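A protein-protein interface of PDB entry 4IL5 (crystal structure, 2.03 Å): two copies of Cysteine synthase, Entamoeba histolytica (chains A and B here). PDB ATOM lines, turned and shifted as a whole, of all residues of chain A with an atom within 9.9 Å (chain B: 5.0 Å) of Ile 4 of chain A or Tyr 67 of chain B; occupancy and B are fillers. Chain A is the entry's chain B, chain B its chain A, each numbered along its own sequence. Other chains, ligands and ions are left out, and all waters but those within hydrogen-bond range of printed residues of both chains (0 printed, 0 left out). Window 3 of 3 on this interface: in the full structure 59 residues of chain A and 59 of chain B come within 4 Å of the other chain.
The backbone carbonyl oxygen (O) of Glu 19 of chain B sits at hydrogen-bond distance from the side-chain hydroxyl (OG) of Ser 7 of chain A, 2.7 Å away.
The side-chain hydroxyl (OH) of Tyr 67 of chain B sits at hydrogen-bond distance from the backbone NH (N) of Ile 4 of chain A (3.3 Å).
The backbone NH (N) of Leu 18 of chain B lies within hydrogen-bond range of the side-chain amide oxygen (OD1) of Asn 16 of chain B (2.9 Å).
N of Glu 19 of chain B sits at hydrogen-bond distance from OD1 of Asn 16 of chain B (3.4 Å).
No position is printed for both chains.
Of the 11 pairs that touch across the chains among the printed residues, none has its exchanged pair printed and touching as well.
Of the 14 printed residues of chain B, 5 touch a printed residue of chain A.
Printed residues of chain A that touch a printed residue of chain B: Ile 4, Ser 5, Ile 6, Ser 7 and Val 27.
Among the printed residues, 11 pairs touch across the chains.
Among the printed residues, no Asp or Glu carboxylate lies within 4 Å of a Lys or Arg side-chain nitrogen of the other chain.
Printed residues of chain B within 4 Å of Ile 4 of chain A: Asn 16, Leu 18, Glu 19, Phe 63 and Tyr 67.
Of the printed residues of chain B, Ile 6 of chain A touches Leu 18, Glu 19 and Phe 63.
Of the printed residues of chain A, Leu 18 of chain B touches Ile 4 (3.8 Å) and Ile 6 (3.7 Å).
Printed residues of chain A within 4 Å of Phe 63 of chain B: Ile 4 and Ile 6.
No residue of chain A comes within 4 Å of Val 66 of chain B.
Of the printed residues of chain A, Tyr 67 of chain B touches Ile 4.
No residue of chain A comes within 4 Å of Ala 69 of chain B.
No residue of chain A comes within 4 Å of Ile 70 of chain B.
The nearest residue of chain A that does not touch Tyr 67 of chain B is Gln 3 of chain A (4.1 Å).
Among the printed residues, pairs that only touch across the chains: Ile 4 of chain A with Asn 16 of chain B (3.6 Å), Ile 4 of chain A with Leu 18 of chain B (3.8 Å), Ile 4 of chain A with Glu 19 of chain B (3.9 Å), Ile 4 of chain A with Phe 63 of chain B (3.7 Å), Ser 5 of chain A with Glu 19 of chain B (3.3 Å), Ile 6 of chain A with Leu 18 of chain B (3.7 Å), Ile 6 of chain A with Glu 19 of chain B (3.7 Å), Ile 6 of chain A with Phe 63 of chain B (3.6 Å) and Val 27 of chain A with Asn 16 of chain B (3.5 Å).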
ATOM      1  N   GLU A   2      -5.845  32.634  -6.187  1.00  0.00           N
ATOM      2  CA  GLU A   2      -4.887  31.875  -7.044  1.00  0.00           C
ATOM      3  C   GLU A   2      -4.554  30.476  -6.452  1.00  0.00           C
ATOM      4  O   GLU A   2      -3.483  29.898  -6.714  1.00  0.00           O
ATOM      5  CB  GLU A   2      -3.643  32.746  -7.367  1.00  0.00           C
ATOM      6  CG  GLU A   2      -2.334  32.462  -6.623  1.00  0.00           C
ATOM      7  CD  GLU A   2      -2.349  32.847  -5.152  1.00  0.00           C
ATOM      8  OE1 GLU A   2      -3.187  32.321  -4.388  1.00  0.00           O
ATOM      9  OE2 GLU A   2      -1.490  33.659  -4.752  1.00  0.00           O
ATOM     10  N   GLN A   3      -5.484  29.953  -5.645  1.00  0.00           N
ATOM     11  CA  GLN A   3      -5.469  28.558  -5.187  1.00  0.00           C
ATOM     12  C   GLN A   3      -5.790  27.662  -6.385  1.00  0.00           C
ATOM     13  O   GLN A   3      -6.656  27.989  -7.202  1.00  0.00           O
ATOM     14  CB  GLN A   3      -6.501  28.345  -4.066  1.00  0.00           C
ATOM     15  CG  GLN A   3      -7.930  28.777  -4.424  1.00  0.00           C
ATOM     16  CD  GLN A   3      -8.843  28.970  -3.218  1.00  0.00           C
ATOM     17  OE1 GLN A   3      -8.560  29.768  -2.317  1.00  0.00           O
ATOM     18  NE2 GLN A   3      -9.961  28.254  -3.208  1.00  0.00           N
ATOM     19  N   ILE A   4      -5.089  26.545  -6.518  1.00  0.00           N
ATOM     20  CA  ILE A   4      -5.318  25.686  -7.680  1.00  0.00           C
ATOM     21  C   ILE A   4      -5.412  24.202  -7.297  1.00  0.00           C
ATOM     22  O   ILE A   4      -4.443  23.589  -6.838  1.00  0.00           O
ATOM     23  CB  ILE A   4      -4.316  25.994  -8.818  1.00  0.00           C
ATOM     24  CG1 ILE A   4      -4.564  25.152 -10.060  1.00  0.00           C
ATOM     25  CG2 ILE A   4      -2.894  25.798  -8.369  1.00  0.00           C
ATOM     26  CD1 ILE A   4      -3.804  25.700 -11.251  1.00  0.00           C
ATOM     27  N   SER A   5      -6.603  23.646  -7.474  1.00  0.00           N
ATOM     28  CA  SER A   5      -6.874  22.278  -7.055  1.00  0.00           C
ATOM     29  C   SER A   5      -6.899  21.382  -8.264  1.00  0.00           C
ATOM     30  O   SER A   5      -7.578  21.668  -9.261  1.00  0.00           O
ATOM     31  CB  SER A   5      -8.217  22.184  -6.334  1.00  0.00           C
ATOM     32  OG  SER A   5      -8.176  22.944  -5.143  1.00  0.00           O
ATOM     33  N   ILE A   6      -6.163  20.288  -8.175  1.00  0.00           N
ATOM     34  CA  ILE A   6      -6.226  19.280  -9.221  1.00  0.00           C
ATOM     35  C   ILE A   6      -7.491  18.426  -9.068  1.00  0.00           C
ATOM     36  O   ILE A   6      -8.261  18.638  -8.135  1.00  0.00           O
ATOM     37  CB  ILE A   6      -4.945  18.432  -9.265  1.00  0.00           C
ATOM     38  CG1 ILE A   6      -4.760  17.665  -7.943  1.00  0.00           C
ATOM     39  CG2 ILE A   6      -3.766  19.333  -9.663  1.00  0.00           C
ATOM     40  CD1 ILE A   6      -3.838  16.464  -8.106  1.00  0.00           C
ATOM     41  N   SER A   7      -7.718  17.490  -9.985  1.00  0.00           N
ATOM     42  CA  SER A   7      -8.970  16.706  -9.995  1.00  0.00           C
ATOM     43  C   SER A   7      -9.051  15.687  -8.889  1.00  0.00           C
ATOM     44  O   SER A   7      -8.033  15.086  -8.532  1.00  0.00           O
ATOM     45  CB  SER A   7      -9.159  16.020 -11.338  1.00  0.00           C
ATOM     46  OG  SER A   7      -9.300  17.025 -12.329  1.00  0.00           O
ATOM     47  N   VAL A  27     -13.201  23.439 -19.831  1.00  0.00           N
ATOM     48  CA  VAL A  27     -12.120  24.293 -19.294  1.00  0.00           C
ATOM     49  C   VAL A  27     -12.245  25.743 -19.794  1.00  0.00           C
ATOM     50  O   VAL A  27     -12.438  25.999 -20.996  1.00  0.00           O
ATOM     51  CB  VAL A  27     -10.739  23.739 -19.728  1.00  0.00           C
ATOM     52  CG1 VAL A  27      -9.589  24.537 -19.099  1.00  0.00           C
ATOM     53  CG2 VAL A  27     -10.624  22.230 -19.372  1.00  0.00           C
ATOM     54  N   HIS A  30      -8.444  31.601 -21.005  1.00  0.00           N
ATOM     55  CA  HIS A  30      -8.111  32.913 -20.450  1.00  0.00           C
ATOM     56  C   HIS A  30      -7.076  33.642 -21.259  1.00  0.00           C
ATOM     57  O   HIS A  30      -7.178  34.857 -21.460  1.00  0.00           O
ATOM     58  CB  HIS A  30      -7.612  32.784 -19.014  1.00  0.00           C
ATOM     59  CG  HIS A  30      -8.631  32.236 -18.074  1.00  0.00           C
ATOM     60  ND1 HIS A  30      -9.672  32.990 -17.574  1.00  0.00           N
ATOM     61  CD2 HIS A  30      -8.771  30.999 -17.541  1.00  0.00           C
ATOM     62  CE1 HIS A  30     -10.412  32.242 -16.776  1.00  0.00           C
ATOM     63  NE2 HIS A  30      -9.878  31.034 -16.726  1.00  0.00           N
ATOM     64  N   ASN B  16      -8.505  26.331 -15.556  1.00  0.00           N
ATOM     65  CA  ASN B  16      -7.421  26.203 -16.523  1.00  0.00           C
ATOM     66  C   ASN B  16      -7.082  24.712 -16.612  1.00  0.00           C
ATOM     67  O   ASN B  16      -7.610  23.905 -15.844  1.00  0.00           O
ATOM     68  CB  ASN B  16      -6.210  27.034 -16.059  1.00  0.00           C
ATOM     69  CG  ASN B  16      -5.710  26.590 -14.711  1.00  0.00           C
ATOM     70  OD1 ASN B  16      -5.372  25.412 -14.518  1.00  0.00           O
ATOM     71  ND2 ASN B  16      -5.707  27.507 -13.745  1.00  0.00           N
ATOM     72  N   LEU B  18      -4.527  22.911 -15.833  1.00  0.00           N
ATOM     73  CA  LEU B  18      -3.844  22.243 -14.706  1.00  0.00           C
ATOM     74  C   LEU B  18      -4.828  21.628 -13.746  1.00  0.00           C
ATOM     75  O   LEU B  18      -4.490  20.686 -13.040  1.00  0.00           O
ATOM     76  CB  LEU B  18      -2.903  23.215 -13.944  1.00  0.00           C
ATOM     77  CG  LEU B  18      -1.909  24.015 -14.790  1.00  0.00           C
ATOM     78  CD1 LEU B  18      -1.044  24.928 -13.902  1.00  0.00           C
ATOM     79  CD2 LEU B  18      -1.038  23.077 -15.627  1.00  0.00           C
ATOM     80  N   GLU B  19      -6.057  22.152 -13.705  1.00  0.00           N
ATOM     81  CA  GLU B  19      -7.059  21.604 -12.792  1.00  0.00           C
ATOM     82  C   GLU B  19      -7.585  20.262 -13.249  1.00  0.00           C
ATOM     83  O   GLU B  19      -8.252  19.564 -12.460  1.00  0.00           O
ATOM     84  CB  GLU B  19      -8.228  22.585 -12.549  1.00  0.00           C
ATOM     85  CG  GLU B  19      -7.797  23.788 -11.733  1.00  0.00           C
ATOM     86  CD  GLU B  19      -8.957  24.696 -11.335  1.00  0.00           C
ATOM     87  OE1 GLU B  19     -10.043  24.684 -11.941  1.00  0.00           O
ATOM     88  OE2 GLU B  19      -8.768  25.430 -10.389  1.00  0.00           O
ATOM     89  N   GLY B  62       5.400  17.892 -13.053  1.00  0.00           N
ATOM     90  CA  GLY B  62       5.675  19.226 -13.546  1.00  0.00           C
ATOM     91  C   GLY B  62       4.778  20.250 -12.876  1.00  0.00           C
ATOM     92  O   GLY B  62       5.227  21.359 -12.482  1.00  0.00           O
ATOM     93  N   PHE B  63       3.509  19.897 -12.720  1.00  0.00           N
ATOM     94  CA  PHE B  63       2.625  20.794 -12.008  1.00  0.00           C
ATOM     95  C   PHE B  63       3.089  21.014 -10.565  1.00  0.00           C
ATOM     96  O   PHE B  63       3.246  22.148 -10.144  1.00  0.00           O
ATOM     97  CB  PHE B  63       1.169  20.306 -11.996  1.00  0.00           C
ATOM     98  CG  PHE B  63       0.307  21.091 -11.065  1.00  0.00           C
ATOM     99  CD1 PHE B  63      -0.061  22.396 -11.381  1.00  0.00           C
ATOM    100  CD2 PHE B  63      -0.071  20.573  -9.845  1.00  0.00           C
ATOM    101  CE1 PHE B  63      -0.829  23.149 -10.509  1.00  0.00           C
ATOM    102  CE2 PHE B  63      -0.845  21.326  -8.957  1.00  0.00           C
ATOM    103  CZ  PHE B  63      -1.225  22.611  -9.294  1.00  0.00           C
ATOM    104  N   ASN B  64       3.261  19.941  -9.792  1.00  0.00           N
ATOM    105  CA  ASN B  64       3.545  20.126  -8.366  1.00  0.00           C
ATOM    106  C   ASN B  64       4.903  20.792  -8.118  1.00  0.00           C
ATOM    107  O   ASN B  64       5.029  21.633  -7.240  1.00  0.00           O
ATOM    108  CB  ASN B  64       3.475  18.830  -7.550  1.00  0.00           C
ATOM    109  CG  ASN B  64       3.217  19.113  -6.085  1.00  0.00           C
ATOM    110  OD1 ASN B  64       2.358  19.937  -5.781  1.00  0.00           O
ATOM    111  ND2 ASN B  64       3.956  18.445  -5.168  1.00  0.00           N
ATOM    112  N   ILE B  65       5.913  20.395  -8.884  1.00  0.00           N
ATOM    113  CA  ILE B  65       7.221  21.059  -8.814  1.00  0.00           C
ATOM    114  C   ILE B  65       7.079  22.588  -8.972  1.00  0.00           C
ATOM    115  O   ILE B  65       7.584  23.356  -8.133  1.00  0.00           O
ATOM    116  CB  ILE B  65       8.223  20.476  -9.834  1.00  0.00           C
ATOM    117  CG1 ILE B  65       8.607  19.043  -9.405  1.00  0.00           C
ATOM    118  CG2 ILE B  65       9.445  21.379  -9.924  1.00  0.00           C
ATOM    119  CD1 ILE B  65       9.628  18.354 -10.305  1.00  0.00           C
ATOM    120  N   VAL B  66       6.399  23.024 -10.030  1.00  0.00           N
ATOM    121  CA  VAL B  66       6.276  24.461 -10.295  1.00  0.00           C
ATOM    122  C   VAL B  66       5.354  25.151  -9.270  1.00  0.00           C
ATOM    123  O   VAL B  66       5.700  26.214  -8.699  1.00  0.00           O
ATOM    124  CB  VAL B  66       5.847  24.733 -11.759  1.00  0.00           C
ATOM    125  CG1 VAL B  66       5.611  26.219 -12.004  1.00  0.00           C
ATOM    126  CG2 VAL B  66       6.904  24.211 -12.717  1.00  0.00           C
ATOM    127  N   TYR B  67       4.206  24.538  -9.003  1.00  0.00           N
ATOM    128  CA  TYR B  67       3.258  25.075  -8.012  1.00  0.00           C
ATOM    129  C   TYR B  67       3.846  25.295  -6.593  1.00  0.00           C
ATOM    130  O   TYR B  67       3.667  26.372  -5.996  1.00  0.00           O
ATOM    131  CB  TYR B  67       2.039  24.170  -7.943  1.00  0.00           C
ATOM    132  CG  TYR B  67       0.903  24.664  -7.095  1.00  0.00           C
ATOM    133  CD1 TYR B  67       0.336  25.927  -7.293  1.00  0.00           C
ATOM    134  CD2 TYR B  67       0.350  23.840  -6.128  1.00  0.00           C
ATOM    135  CE1 TYR B  67      -0.727  26.367  -6.516  1.00  0.00           C
ATOM    136  CE2 TYR B  67      -0.736  24.249  -5.362  1.00  0.00           C
ATOM    137  CZ  TYR B  67      -1.266  25.513  -5.553  1.00  0.00           C
ATOM    138  OH  TYR B  67      -2.336  25.904  -4.774  1.00  0.00           O
ATOM    139  N   GLN B  68       4.494  24.255  -6.057  1.00  0.00           N
ATOM    140  CA  GLN B  68       5.163  24.326  -4.765  1.00  0.00           C
ATOM    141  C   GLN B  68       6.274  25.345  -4.729  1.00  0.00           C
ATOM    142  O   GLN B  68       6.455  26.040  -3.713  1.00  0.00           O
ATOM    143  CB  GLN B  68       5.744  22.978  -4.400  1.00  0.00           C
ATOM    144  CG  GLN B  68       4.760  22.075  -3.724  1.00  0.00           C
ATOM    145  CD  GLN B  68       4.161  22.730  -2.499  1.00  0.00           C
ATOM    146  OE1 GLN B  68       4.816  23.487  -1.750  1.00  0.00           O
ATOM    147  NE2 GLN B  68       2.921  22.469  -2.301  1.00  0.00           N
ATOM    148  N   ALA B  69       7.015  25.443  -5.830  1.00  0.00           N
ATOM    149  CA  ALA B  69       8.098  26.404  -5.904  1.00  0.00           C
ATOM    150  C   ALA B  69       7.535  27.842  -5.846  1.00  0.00           C
ATOM    151  O   ALA B  69       8.083  28.716  -5.151  1.00  0.00           O
ATOM    152  CB  ALA B  69       8.917  26.182  -7.155  1.00  0.00           C
ATOM    153  N   ILE B  70       6.435  28.068  -6.574  1.00  0.00           N
ATOM    154  CA  ILE B  70       5.735  29.344  -6.525  1.00  0.00           C
ATOM    155  C   ILE B  70       5.203  29.604  -5.120  1.00  0.00           C
ATOM    156  O   ILE B  70       5.408  30.674  -4.597  1.00  0.00           O
ATOM    157  CB  ILE B  70       4.618  29.441  -7.579  1.00  0.00           C
ATOM    158  CG1 ILE B  70       5.238  29.580  -8.968  1.00  0.00           C
ATOM    159  CG2 ILE B  70       3.688  30.619  -7.267  1.00  0.00           C
ATOM    160  CD1 ILE B  70       4.268  29.307 -10.103  1.00  0.00           C
ATOM    161  N   LYS B  71       4.565  28.622  -4.497  1.00  0.00           N
ATOM    162  CA  LYS B  71       4.067  28.802  -3.151  1.00  0.00           C
ATOM    163  C   LYS B  71       5.168  29.051  -2.091  1.00  0.00           C
ATOM    164  O   LYS B  71       4.931  29.802  -1.138  1.00  0.00           O
ATOM    165  CB  LYS B  71       3.222  27.623  -2.730  1.00  0.00           C
ATOM    166  CG  LYS B  71       1.850  27.585  -3.385  1.00  0.00           C
ATOM    167  CD  LYS B  71       1.235  26.197  -3.243  1.00  0.00           C
ATOM    168  CE  LYS B  71       1.077  25.801  -1.793  1.00  0.00           C
ATOM    169  NZ  LYS B  71       0.616  24.389  -1.665  1.00  0.00           N
ATOM    170  N   PHE B 100       1.152  29.124 -15.700  1.00  0.00           N
ATOM    171  CA  PHE B 100       1.601  30.035 -14.639  1.00  0.00           C
ATOM    172  C   PHE B 100       2.265  31.299 -15.204  1.00  0.00           C
ATOM    173  O   PHE B 100       2.468  32.261 -14.487  1.00  0.00           O
ATOM    174  CB  PHE B 100       2.540  29.342 -13.656  1.00  0.00           C
ATOM    175  CG  PHE B 100       1.864  28.391 -12.717  1.00  0.00           C
ATOM    176  CD1 PHE B 100       0.966  28.846 -11.759  1.00  0.00           C
ATOM    177  CD2 PHE B 100       2.167  27.029 -12.762  1.00  0.00           C
ATOM    178  CE1 PHE B 100       0.358  27.950 -10.885  1.00  0.00           C
ATOM    179  CE2 PHE B 100       1.573  26.145 -11.895  1.00  0.00           C
ATOM    180  CZ  PHE B 100       0.663  26.594 -10.958  1.00  0.00           C
